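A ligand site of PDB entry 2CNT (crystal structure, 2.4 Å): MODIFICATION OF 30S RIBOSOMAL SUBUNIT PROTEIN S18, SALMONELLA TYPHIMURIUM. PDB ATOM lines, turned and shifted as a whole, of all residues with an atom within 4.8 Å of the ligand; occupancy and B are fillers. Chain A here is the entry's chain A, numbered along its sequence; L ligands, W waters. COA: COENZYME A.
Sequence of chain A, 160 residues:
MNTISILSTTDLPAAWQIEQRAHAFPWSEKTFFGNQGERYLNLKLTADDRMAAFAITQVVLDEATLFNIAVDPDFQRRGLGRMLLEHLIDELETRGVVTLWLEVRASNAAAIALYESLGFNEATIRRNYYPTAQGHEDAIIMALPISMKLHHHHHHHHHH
N of Ile 69 sits close to S1P of the ligand, at 3.8 Å.
An oxygen (O2A) of the ligand sits at hydrogen-bond distance from the backbone NH (N) of Arg 78, 3.1 Å away.
The guanidinium group of Arg 77 is in hydrogen-bond range of an oxygen (O2B) of the ligand (3.1 Å).
The side-chain amide nitrogen of Gln 76 is in hydrogen-bond range of an oxygen (O9P) of the ligand, at 3.4 Å.
ND2 of Asn 108 sits at hydrogen-bond distance from O5P of the ligand (3.1 Å).
The backbone carbonyl oxygen of Ile 69 lies within hydrogen-bond range of a nitrogen (N4P) of the ligand, at 2.8 Å.
The backbone NH (N) of Arg 82 is in hydrogen-bond range of an oxygen (O1A) of the ligand (2.9 Å).
The backbone NH (N) of Leu 114 sits at hydrogen-bond distance from an oxygen (O4B) of the ligand (3.4 Å).
An oxygen (O4A) of the ligand sits at hydrogen-bond distance from the backbone NH (N) of Gly 81, at 2.7 Å.
The backbone NH of Arg 77 is in hydrogen-bond range of an oxygen (O5A) of the ligand, at 3.0 Å.
An oxygen (O9P) of the ligand is in hydrogen-bond range of the backbone NH (N) of Val 71, 2.7 Å away.
The backbone NH (N) of Gly 79 lies within hydrogen-bond range of an oxygen (O2A) of the ligand, at 2.7 Å.
The guanidinium group (NH2) of Arg 82 is in salt-bridge range of an oxygen (O9A) of the ligand, at 3.1 Å.
Water W2 bridges OH of Tyr 115 (3.0 Å) and S1P of the ligand (3.5 Å).
The backbone carbonyl oxygen of Ala 110 sits close to an oxygen (O4B) of the ligand.
O of Ala 22 touches C7P of the ligand, at 3.2 Å.
His 23 touches the ligand.
Ala 70 touches the ligand (CA to O9P, 3.5 Å).
N of Leu 80 touches O4A of the ligand (3.6 Å).
Ala 111 touches the ligand.
Ala 113 touches the ligand.
Tyr 115 touches the ligand (OH to C3P, 3.3 Å).
Hydrophobic or aromatic side chains that line the ligand: His 23, Ile 69, Val 71, Ala 110, Ala 111, Ala 113 and Leu 114.
Within 4 Å of the ligand: Ala 22, His 23, Ile 69, Ala 70, Val 71, Gln 76, Arg 77, Arg 78, Gly 79, Leu 80, Gly 81, Arg 82, Asn 108, Ala 110, Ala 111, Ala 113, Leu 114 and Tyr 115.
The side-chain hydroxyl of Ser 117 lies within hydrogen-bond range of the guanidinium group of Arg 82 (2.9 Å).
OD1 of Asn 68 lies within hydrogen-bond range of NE2 of His 23 (2.6 Å).
NE2 of Gln 76 sits at hydrogen-bond distance from O of Val 71, at 2.8 Å.
OD1 of Asn 108 is in hydrogen-bond range of N of Ala 111 (3.4 Å).
The backbone carbonyl oxygen (O) of Ala 113 is in hydrogen-bond range of the side-chain hydroxyl (OG) of Ser 117 (3.4 Å).
The backbone carbonyl oxygen of Leu 114 is in hydrogen-bond range of the side-chain hydroxyl of Ser 117 (2.6 Å).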
ATOM      1  N   ALA A  22      15.655 -32.394 -27.269  1.00  0.00           N
ATOM      2  CA  ALA A  22      15.335 -31.820 -25.954  1.00  0.00           C
ATOM      3  C   ALA A  22      14.115 -32.451 -25.325  1.00  0.00           C
ATOM      4  O   ALA A  22      14.157 -32.811 -24.150  1.00  0.00           O
ATOM      5  CB  ALA A  22      15.165 -30.299 -26.031  1.00  0.00           C
ATOM      6  N   HIS A  23      13.041 -32.620 -26.108  1.00  0.00           N
ATOM      7  CA  HIS A  23      11.755 -33.085 -25.590  1.00  0.00           C
ATOM      8  C   HIS A  23      11.668 -34.584 -25.363  1.00  0.00           C
ATOM      9  O   HIS A  23      12.080 -35.357 -26.228  1.00  0.00           O
ATOM     10  CB  HIS A  23      10.635 -32.660 -26.542  1.00  0.00           C
ATOM     11  CG  HIS A  23      10.307 -31.211 -26.442  1.00  0.00           C
ATOM     12  ND1 HIS A  23       9.482 -30.716 -25.460  1.00  0.00           N
ATOM     13  CD2 HIS A  23      10.732 -30.157 -27.168  1.00  0.00           C
ATOM     14  CE1 HIS A  23       9.376 -29.396 -25.616  1.00  0.00           C
ATOM     15  NE2 HIS A  23      10.121 -29.037 -26.642  1.00  0.00           N
ATOM     16  N   PHE A  67       3.529 -22.601 -26.242  1.00  0.00           N
ATOM     17  CA  PHE A  67       3.354 -23.955 -26.738  1.00  0.00           C
ATOM     18  C   PHE A  67       4.588 -24.811 -26.526  1.00  0.00           C
ATOM     19  O   PHE A  67       4.472 -26.034 -26.344  1.00  0.00           O
ATOM     20  CB  PHE A  67       2.972 -23.947 -28.221  1.00  0.00           C
ATOM     21  CG  PHE A  67       1.567 -23.511 -28.471  1.00  0.00           C
ATOM     22  CD1 PHE A  67       0.514 -24.026 -27.709  1.00  0.00           C
ATOM     23  CD2 PHE A  67       1.288 -22.575 -29.453  1.00  0.00           C
ATOM     24  CE1 PHE A  67      -0.815 -23.624 -27.939  1.00  0.00           C
ATOM     25  CE2 PHE A  67      -0.045 -22.177 -29.696  1.00  0.00           C
ATOM     26  CZ  PHE A  67      -1.090 -22.689 -28.938  1.00  0.00           C
ATOM     27  N   ASN A  68       5.747 -24.159 -26.509  1.00  0.00           N
ATOM     28  CA  ASN A  68       7.010 -24.857 -26.496  1.00  0.00           C
ATOM     29  C   ASN A  68       8.145 -23.981 -25.973  1.00  0.00           C
ATOM     30  O   ASN A  68       8.327 -22.862 -26.404  1.00  0.00           O
ATOM     31  CB  ASN A  68       7.335 -25.317 -27.932  1.00  0.00           C
ATOM     32  CG  ASN A  68       8.284 -26.525 -27.990  1.00  0.00           C
ATOM     33  OD1 ASN A  68       9.252 -26.646 -27.203  1.00  0.00           O
ATOM     34  ND2 ASN A  68       8.046 -27.391 -28.950  1.00  0.00           N
ATOM     35  N   ILE A  69       8.930 -24.510 -25.036  1.00  0.00           N
ATOM     36  CA  ILE A  69      10.256 -23.980 -24.760  1.00  0.00           C
ATOM     37  C   ILE A  69      11.184 -25.188 -24.788  1.00  0.00           C
ATOM     38  O   ILE A  69      10.862 -26.232 -24.215  1.00  0.00           O
ATOM     39  CB  ILE A  69      10.327 -23.180 -23.412  1.00  0.00           C
ATOM     40  CG1 ILE A  69      11.749 -22.727 -23.098  1.00  0.00           C
ATOM     41  CG2 ILE A  69       9.811 -24.009 -22.239  1.00  0.00           C
ATOM     42  CD1 ILE A  69      12.112 -21.408 -23.673  1.00  0.00           C
ATOM     43  N   ALA A  70      12.303 -25.081 -25.492  1.00  0.00           N
ATOM     44  CA  ALA A  70      13.298 -26.151 -25.489  1.00  0.00           C
ATOM     45  C   ALA A  70      14.678 -25.552 -25.529  1.00  0.00           C
ATOM     46  O   ALA A  70      14.938 -24.579 -26.251  1.00  0.00           O
ATOM     47  CB  ALA A  70      13.099 -27.119 -26.650  1.00  0.00           C
ATOM     48  N   VAL A  71      15.557 -26.148 -24.721  1.00  0.00           N
ATOM     49  CA  VAL A  71      16.960 -25.784 -24.612  1.00  0.00           C
ATOM     50  C   VAL A  71      17.722 -27.018 -25.025  1.00  0.00           C
ATOM     51  O   VAL A  71      17.459 -28.133 -24.532  1.00  0.00           O
ATOM     52  CB  VAL A  71      17.358 -25.299 -23.180  1.00  0.00           C
ATOM     53  CG1 VAL A  71      18.831 -25.012 -23.081  1.00  0.00           C
ATOM     54  CG2 VAL A  71      16.546 -24.035 -22.809  1.00  0.00           C
ATOM     55  N   PHE A  75      23.249 -27.300 -23.635  1.00  0.00           N
ATOM     56  CA  PHE A  75      23.165 -25.963 -23.060  1.00  0.00           C
ATOM     57  C   PHE A  75      22.337 -25.841 -21.776  1.00  0.00           C
ATOM     58  O   PHE A  75      22.173 -24.737 -21.257  1.00  0.00           O
ATOM     59  CB  PHE A  75      22.607 -24.972 -24.101  1.00  0.00           C
ATOM     60  CG  PHE A  75      23.623 -24.531 -25.115  1.00  0.00           C
ATOM     61  CD1 PHE A  75      24.538 -23.534 -24.811  1.00  0.00           C
ATOM     62  CD2 PHE A  75      23.666 -25.128 -26.368  1.00  0.00           C
ATOM     63  CE1 PHE A  75      25.484 -23.121 -25.746  1.00  0.00           C
ATOM     64  CE2 PHE A  75      24.602 -24.733 -27.317  1.00  0.00           C
ATOM     65  CZ  PHE A  75      25.516 -23.727 -27.008  1.00  0.00           C
ATOM     66  N   GLN A  76      21.825 -26.971 -21.279  1.00  0.00           N
ATOM     67  CA  GLN A  76      20.870 -26.958 -20.167  1.00  0.00           C
ATOM     68  C   GLN A  76      21.507 -26.639 -18.795  1.00  0.00           C
ATOM     69  O   GLN A  76      22.718 -26.717 -18.639  1.00  0.00           O
ATOM     70  CB  GLN A  76      20.063 -28.268 -20.156  1.00  0.00           C
ATOM     71  CG  GLN A  76      19.071 -28.361 -21.312  1.00  0.00           C
ATOM     72  CD  GLN A  76      18.272 -29.664 -21.329  1.00  0.00           C
ATOM     73  OE1 GLN A  76      18.372 -30.476 -20.407  1.00  0.00           O
ATOM     74  NE2 GLN A  76      17.461 -29.862 -22.378  1.00  0.00           N
ATOM     75  N   ARG A  77      20.679 -26.238 -17.817  1.00  0.00           N
ATOM     76  CA  ARG A  77      21.177 -25.908 -16.469  1.00  0.00           C
ATOM     77  C   ARG A  77      22.210 -24.779 -16.484  1.00  0.00           C
ATOM     78  O   ARG A  77      23.126 -24.761 -15.684  1.00  0.00           O
ATOM     79  CB  ARG A  77      21.789 -27.129 -15.783  1.00  0.00           C
ATOM     80  CG  ARG A  77      20.850 -28.311 -15.582  1.00  0.00           C
ATOM     81  CD  ARG A  77      19.924 -28.029 -14.428  1.00  0.00           C
ATOM     82  NE  ARG A  77      19.752 -29.198 -13.559  1.00  0.00           N
ATOM     83  CZ  ARG A  77      19.457 -29.084 -12.248  1.00  0.00           C
ATOM     84  NH1 ARG A  77      19.305 -27.834 -11.653  1.00  0.00           N
ATOM     85  NH2 ARG A  77      19.307 -30.209 -11.535  1.00  0.00           N
ATOM     86  N   ARG A  78      22.021 -23.826 -17.390  1.00  0.00           N
ATOM     87  CA  ARG A  78      22.986 -22.746 -17.594  1.00  0.00           C
ATOM     88  C   ARG A  78      22.300 -21.379 -17.534  1.00  0.00           C
ATOM     89  O   ARG A  78      22.938 -20.348 -17.706  1.00  0.00           O
ATOM     90  CB  ARG A  78      23.701 -22.987 -18.933  1.00  0.00           C
ATOM     91  CG  ARG A  78      24.729 -21.955 -19.382  1.00  0.00           C
ATOM     92  CD  ARG A  78      25.515 -22.447 -20.589  1.00  0.00           C
ATOM     93  NE  ARG A  78      25.965 -23.834 -20.427  1.00  0.00           N
ATOM     94  CZ  ARG A  78      26.713 -24.491 -21.312  1.00  0.00           C
ATOM     95  NH1 ARG A  78      27.098 -23.893 -22.446  1.00  0.00           N
ATOM     96  NH2 ARG A  78      27.070 -25.757 -21.088  1.00  0.00           N
ATOM     97  N   GLY A  79      21.000 -21.387 -17.264  1.00  0.00           N
ATOM     98  CA  GLY A  79      20.216 -20.152 -17.142  1.00  0.00           C
ATOM     99  C   GLY A  79      19.546 -19.671 -18.418  1.00  0.00           C
ATOM    100  O   GLY A  79      18.808 -18.712 -18.414  1.00  0.00           O
ATOM    101  N   LEU A  80      19.781 -20.376 -19.519  1.00  0.00           N
ATOM    102  CA  LEU A  80      19.324 -19.890 -20.831  1.00  0.00           C
ATOM    103  C   LEU A  80      17.825 -20.037 -21.083  1.00  0.00           C
ATOM    104  O   LEU A  80      17.240 -19.220 -21.787  1.00  0.00           O
ATOM    105  CB  LEU A  80      20.154 -20.533 -21.958  1.00  0.00           C
ATOM    106  CG  LEU A  80      21.655 -20.386 -21.800  1.00  0.00           C
ATOM    107  CD1 LEU A  80      22.355 -21.103 -22.946  1.00  0.00           C
ATOM    108  CD2 LEU A  80      22.114 -18.930 -21.694  1.00  0.00           C
ATOM    109  N   GLY A  81      17.204 -21.053 -20.515  1.00  0.00           N
ATOM    110  CA  GLY A  81      15.751 -21.225 -20.600  1.00  0.00           C
ATOM    111  C   GLY A  81      15.021 -20.139 -19.853  1.00  0.00           C
ATOM    112  O   GLY A  81      14.070 -19.575 -20.368  1.00  0.00           O
ATOM    113  N   ARG A  82      15.472 -19.827 -18.641  1.00  0.00           N
ATOM    114  CA  ARG A  82      14.970 -18.692 -17.880  1.00  0.00           C
ATOM    115  C   ARG A  82      15.153 -17.388 -18.637  1.00  0.00           C
ATOM    116  O   ARG A  82      14.228 -16.588 -18.705  1.00  0.00           O
ATOM    117  CB  ARG A  82      15.651 -18.613 -16.498  1.00  0.00           C
ATOM    118  CG  ARG A  82      15.103 -17.508 -15.610  1.00  0.00           C
ATOM    119  CD  ARG A  82      15.840 -17.420 -14.279  1.00  0.00           C
ATOM    120  NE  ARG A  82      15.246 -18.362 -13.331  1.00  0.00           N
ATOM    121  CZ  ARG A  82      15.832 -19.474 -12.881  1.00  0.00           C
ATOM    122  NH1 ARG A  82      17.068 -19.822 -13.253  1.00  0.00           N
ATOM    123  NH2 ARG A  82      15.161 -20.245 -12.034  1.00  0.00           N
ATOM    124  N   VAL A 104       1.773 -28.387 -19.050  1.00  0.00           N
ATOM    125  CA  VAL A 104       2.994 -29.187 -18.855  1.00  0.00           C
ATOM    126  C   VAL A 104       2.666 -30.551 -18.180  1.00  0.00           C
ATOM    127  O   VAL A 104       1.829 -30.631 -17.298  1.00  0.00           O
ATOM    128  CB  VAL A 104       4.135 -28.395 -18.084  1.00  0.00           C
ATOM    129  CG1 VAL A 104       3.695 -27.957 -16.705  1.00  0.00           C
ATOM    130  CG2 VAL A 104       5.433 -29.200 -17.988  1.00  0.00           C
ATOM    131  N   ASN A 108       7.337 -33.509 -15.468  1.00  0.00           N
ATOM    132  CA  ASN A 108       8.412 -32.683 -16.012  1.00  0.00           C
ATOM    133  C   ASN A 108       8.921 -31.720 -14.952  1.00  0.00           C
ATOM    134  O   ASN A 108       8.543 -30.558 -14.929  1.00  0.00           O
ATOM    135  CB  ASN A 108       7.922 -31.930 -17.262  1.00  0.00           C
ATOM    136  CG  ASN A 108       9.062 -31.432 -18.139  1.00  0.00           C
ATOM    137  OD1 ASN A 108      10.202 -31.264 -17.674  1.00  0.00           O
ATOM    138  ND2 ASN A 108       8.767 -31.181 -19.393  1.00  0.00           N
ATOM    139  N   ALA A 109       9.762 -32.242 -14.067  1.00  0.00           N
ATOM    140  CA  ALA A 109      10.268 -31.530 -12.899  1.00  0.00           C
ATOM    141  C   ALA A 109      11.063 -30.246 -13.211  1.00  0.00           C
ATOM    142  O   ALA A 109      10.993 -29.270 -12.462  1.00  0.00           O
ATOM    143  CB  ALA A 109      11.111 -32.481 -12.038  1.00  0.00           C
ATOM    144  N   ALA A 110      11.813 -30.298 -14.308  1.00  0.00           N
ATOM    145  CA  ALA A 110      12.711 -29.237 -14.766  1.00  0.00           C
ATOM    146  C   ALA A 110      11.921 -28.040 -15.317  1.00  0.00           C
ATOM    147  O   ALA A 110      12.171 -26.880 -14.946  1.00  0.00           O
ATOM    148  CB  ALA A 110      13.629 -29.794 -15.849  1.00  0.00           C
ATOM    149  N   ALA A 111      11.003 -28.340 -16.241  1.00  0.00           N
ATOM    150  CA  ALA A 111      10.031 -27.381 -16.760  1.00  0.00           C
ATOM    151  C   ALA A 111       9.214 -26.753 -15.624  1.00  0.00           C
ATOM    152  O   ALA A 111       9.197 -25.511 -15.483  1.00  0.00           O
ATOM    153  CB  ALA A 111       9.126 -28.051 -17.796  1.00  0.00           C
ATOM    154  N   ALA A 113       9.820 -26.506 -12.478  1.00  0.00           N
ATOM    155  CA  ALA A 113      10.676 -25.636 -11.656  1.00  0.00           C
ATOM    156  C   ALA A 113      10.997 -24.306 -12.355  1.00  0.00           C
ATOM    157  O   ALA A 113      10.922 -23.236 -11.718  1.00  0.00           O
ATOM    158  CB  ALA A 113      11.974 -26.355 -11.223  1.00  0.00           C
ATOM    159  N   LEU A 114      11.349 -24.363 -13.641  1.00  0.00           N
ATOM    160  CA  LEU A 114      11.575 -23.158 -14.438  1.00  0.00           C
ATOM    161  C   LEU A 114      10.387 -22.197 -14.350  1.00  0.00           C
ATOM    162  O   LEU A 114      10.570 -20.988 -14.187  1.00  0.00           O
ATOM    163  CB  LEU A 114      11.853 -23.510 -15.907  1.00  0.00           C
ATOM    164  CG  LEU A 114      11.918 -22.328 -16.904  1.00  0.00           C
ATOM    165  CD1 LEU A 114      13.021 -21.323 -16.536  1.00  0.00           C
ATOM    166  CD2 LEU A 114      12.048 -22.798 -18.348  1.00  0.00           C
ATOM    167  N   TYR A 115       9.182 -22.759 -14.464  1.00  0.00           N
ATOM    168  CA  TYR A 115       7.957 -21.983 -14.494  1.00  0.00           C
ATOM    169  C   TYR A 115       7.649 -21.438 -13.109  1.00  0.00           C
ATOM    170  O   TYR A 115       7.192 -20.319 -12.967  1.00  0.00           O
ATOM    171  CB  TYR A 115       6.766 -22.812 -15.032  1.00  0.00           C
ATOM    172  CG  TYR A 115       6.973 -23.436 -16.380  1.00  0.00           C
ATOM    173  CD1 TYR A 115       7.680 -22.771 -17.388  1.00  0.00           C
ATOM    174  CD2 TYR A 115       6.436 -24.680 -16.672  1.00  0.00           C
ATOM    175  CE1 TYR A 115       7.875 -23.357 -18.669  1.00  0.00           C
ATOM    176  CE2 TYR A 115       6.603 -25.277 -17.924  1.00  0.00           C
ATOM    177  CZ  TYR A 115       7.328 -24.607 -18.915  1.00  0.00           C
ATOM    178  OH  TYR A 115       7.497 -25.192 -20.149  1.00  0.00           O
ATOM    179  N   SER A 117       9.806 -20.499 -10.903  1.00  0.00           N
ATOM    180  CA  SER A 117      10.752 -19.400 -10.654  1.00  0.00           C
ATOM    181  C   SER A 117      10.352 -18.125 -11.377  1.00  0.00           C
ATOM    182  O   SER A 117      10.681 -17.021 -10.931  1.00  0.00           O
ATOM    183  CB  SER A 117      12.190 -19.791 -11.010  1.00  0.00           C
ATOM    184  OG  SER A 117      12.309 -20.177 -12.363  1.00  0.00           O
HETATM  185  N1A COA L   1      15.984 -30.845 -12.731  1.00  0.00           N
HETATM  186  C2A COA L   1      15.517 -30.062 -11.768  1.00  0.00           C
HETATM  187  N3A COA L   1      15.493 -28.739 -11.904  1.00  0.00           N
HETATM  188  C4A COA L   1      15.925 -28.149 -13.050  1.00  0.00           C
HETATM  189  C5A COA L   1      16.415 -28.945 -14.079  1.00  0.00           C
HETATM  190  C6A COA L   1      16.435 -30.328 -13.888  1.00  0.00           C
HETATM  191  N6A COA L   1      16.895 -31.124 -14.854  1.00  0.00           N
HETATM  192  N7A COA L   1      16.767 -28.136 -15.084  1.00  0.00           N
HETATM  193  C8A COA L   1      16.508 -26.888 -14.706  1.00  0.00           C
HETATM  194  N9A COA L   1      15.991 -26.898 -13.477  1.00  0.00           N
HETATM  195  C1B COA L   1      15.586 -25.703 -12.706  1.00  0.00           C
HETATM  196  C2B COA L   1      16.842 -24.803 -12.558  1.00  0.00           C
HETATM  197  O2B COA L   1      17.705 -25.136 -11.434  1.00  0.00           O
HETATM  198  C3B COA L   1      16.202 -23.413 -12.481  1.00  0.00           C
HETATM  199  O3B COA L   1      15.523 -23.244 -11.245  1.00  0.00           O
HETATM  200  P3B COA L   1      16.331 -22.586  -9.994  1.00  0.00           P
HETATM  201  O7A COA L   1      17.768 -21.964 -10.616  1.00  0.00           O
HETATM  202  O8A COA L   1      16.763 -23.898  -9.071  1.00  0.00           O
HETATM  203  O9A COA L   1      15.482 -21.588  -9.257  1.00  0.00           O
HETATM  204  C4B COA L   1      15.136 -23.514 -13.573  1.00  0.00           C
HETATM  205  O4B COA L   1      14.745 -24.933 -13.603  1.00  0.00           O
HETATM  206  C5B COA L   1      15.545 -22.977 -14.944  1.00  0.00           C
HETATM  207  O5B COA L   1      16.957 -22.884 -15.122  1.00  0.00           O
HETATM  208  P1A COA L   1      17.608 -22.846 -16.598  1.00  0.00           P
HETATM  209  O1A COA L   1      17.232 -21.509 -17.108  1.00  0.00           O
HETATM  210  O2A COA L   1      19.062 -23.198 -16.558  1.00  0.00           O
HETATM  211  O3A COA L   1      16.858 -24.079 -17.384  1.00  0.00           O
HETATM  212  P2A COA L   1      17.263 -24.581 -18.900  1.00  0.00           P
HETATM  213  O4A COA L   1      17.993 -23.522 -19.651  1.00  0.00           O
HETATM  214  O5A COA L   1      17.877 -25.933 -18.818  1.00  0.00           O
HETATM  215  O6A COA L   1      15.802 -24.824 -19.498  1.00  0.00           O
HETATM  216  CBP COA L   1      14.026 -26.486 -19.874  1.00  0.00           C
HETATM  217  CCP COA L   1      14.842 -25.699 -18.822  1.00  0.00           C
HETATM  218  CDP COA L   1      12.768 -26.994 -19.169  1.00  0.00           C
HETATM  219  CEP COA L   1      13.605 -25.532 -21.023  1.00  0.00           C
HETATM  220  CAP COA L   1      14.943 -27.646 -20.394  1.00  0.00           C
HETATM  221  OAP COA L   1      15.100 -28.624 -19.382  1.00  0.00           O
HETATM  222  C9P COA L   1      14.444 -28.342 -21.679  1.00  0.00           C
HETATM  223  O9P COA L   1      14.758 -27.925 -22.796  1.00  0.00           O
HETATM  224  N8P COA L   1      13.661 -29.420 -21.477  1.00  0.00           N
HETATM  225  C7P COA L   1      13.110 -30.169 -22.601  1.00  0.00           C
HETATM  226  C6P COA L   1      12.014 -29.338 -23.279  1.00  0.00           C
HETATM  227  C5P COA L   1      10.791 -29.277 -22.360  1.00  0.00           C
HETATM  228  O5P COA L   1      10.429 -30.307 -21.804  1.00  0.00           O
HETATM  229  N4P COA L   1      10.200 -28.069 -22.248  1.00  0.00           N
HETATM  230  C3P COA L   1       9.033 -27.783 -21.381  1.00  0.00           C
HETATM  231  C2P COA L   1       7.675 -28.222 -21.924  1.00  0.00           C
HETATM  232  S1P COA L   1       7.416 -27.646 -23.635  1.00  0.00           S
HETATM  233  O   HOH W   1      20.706 -23.211 -20.051  1.00  0.00           O
HETATM  234  O   HOH W   2       5.048 -26.559 -21.232  1.00  0.00           O
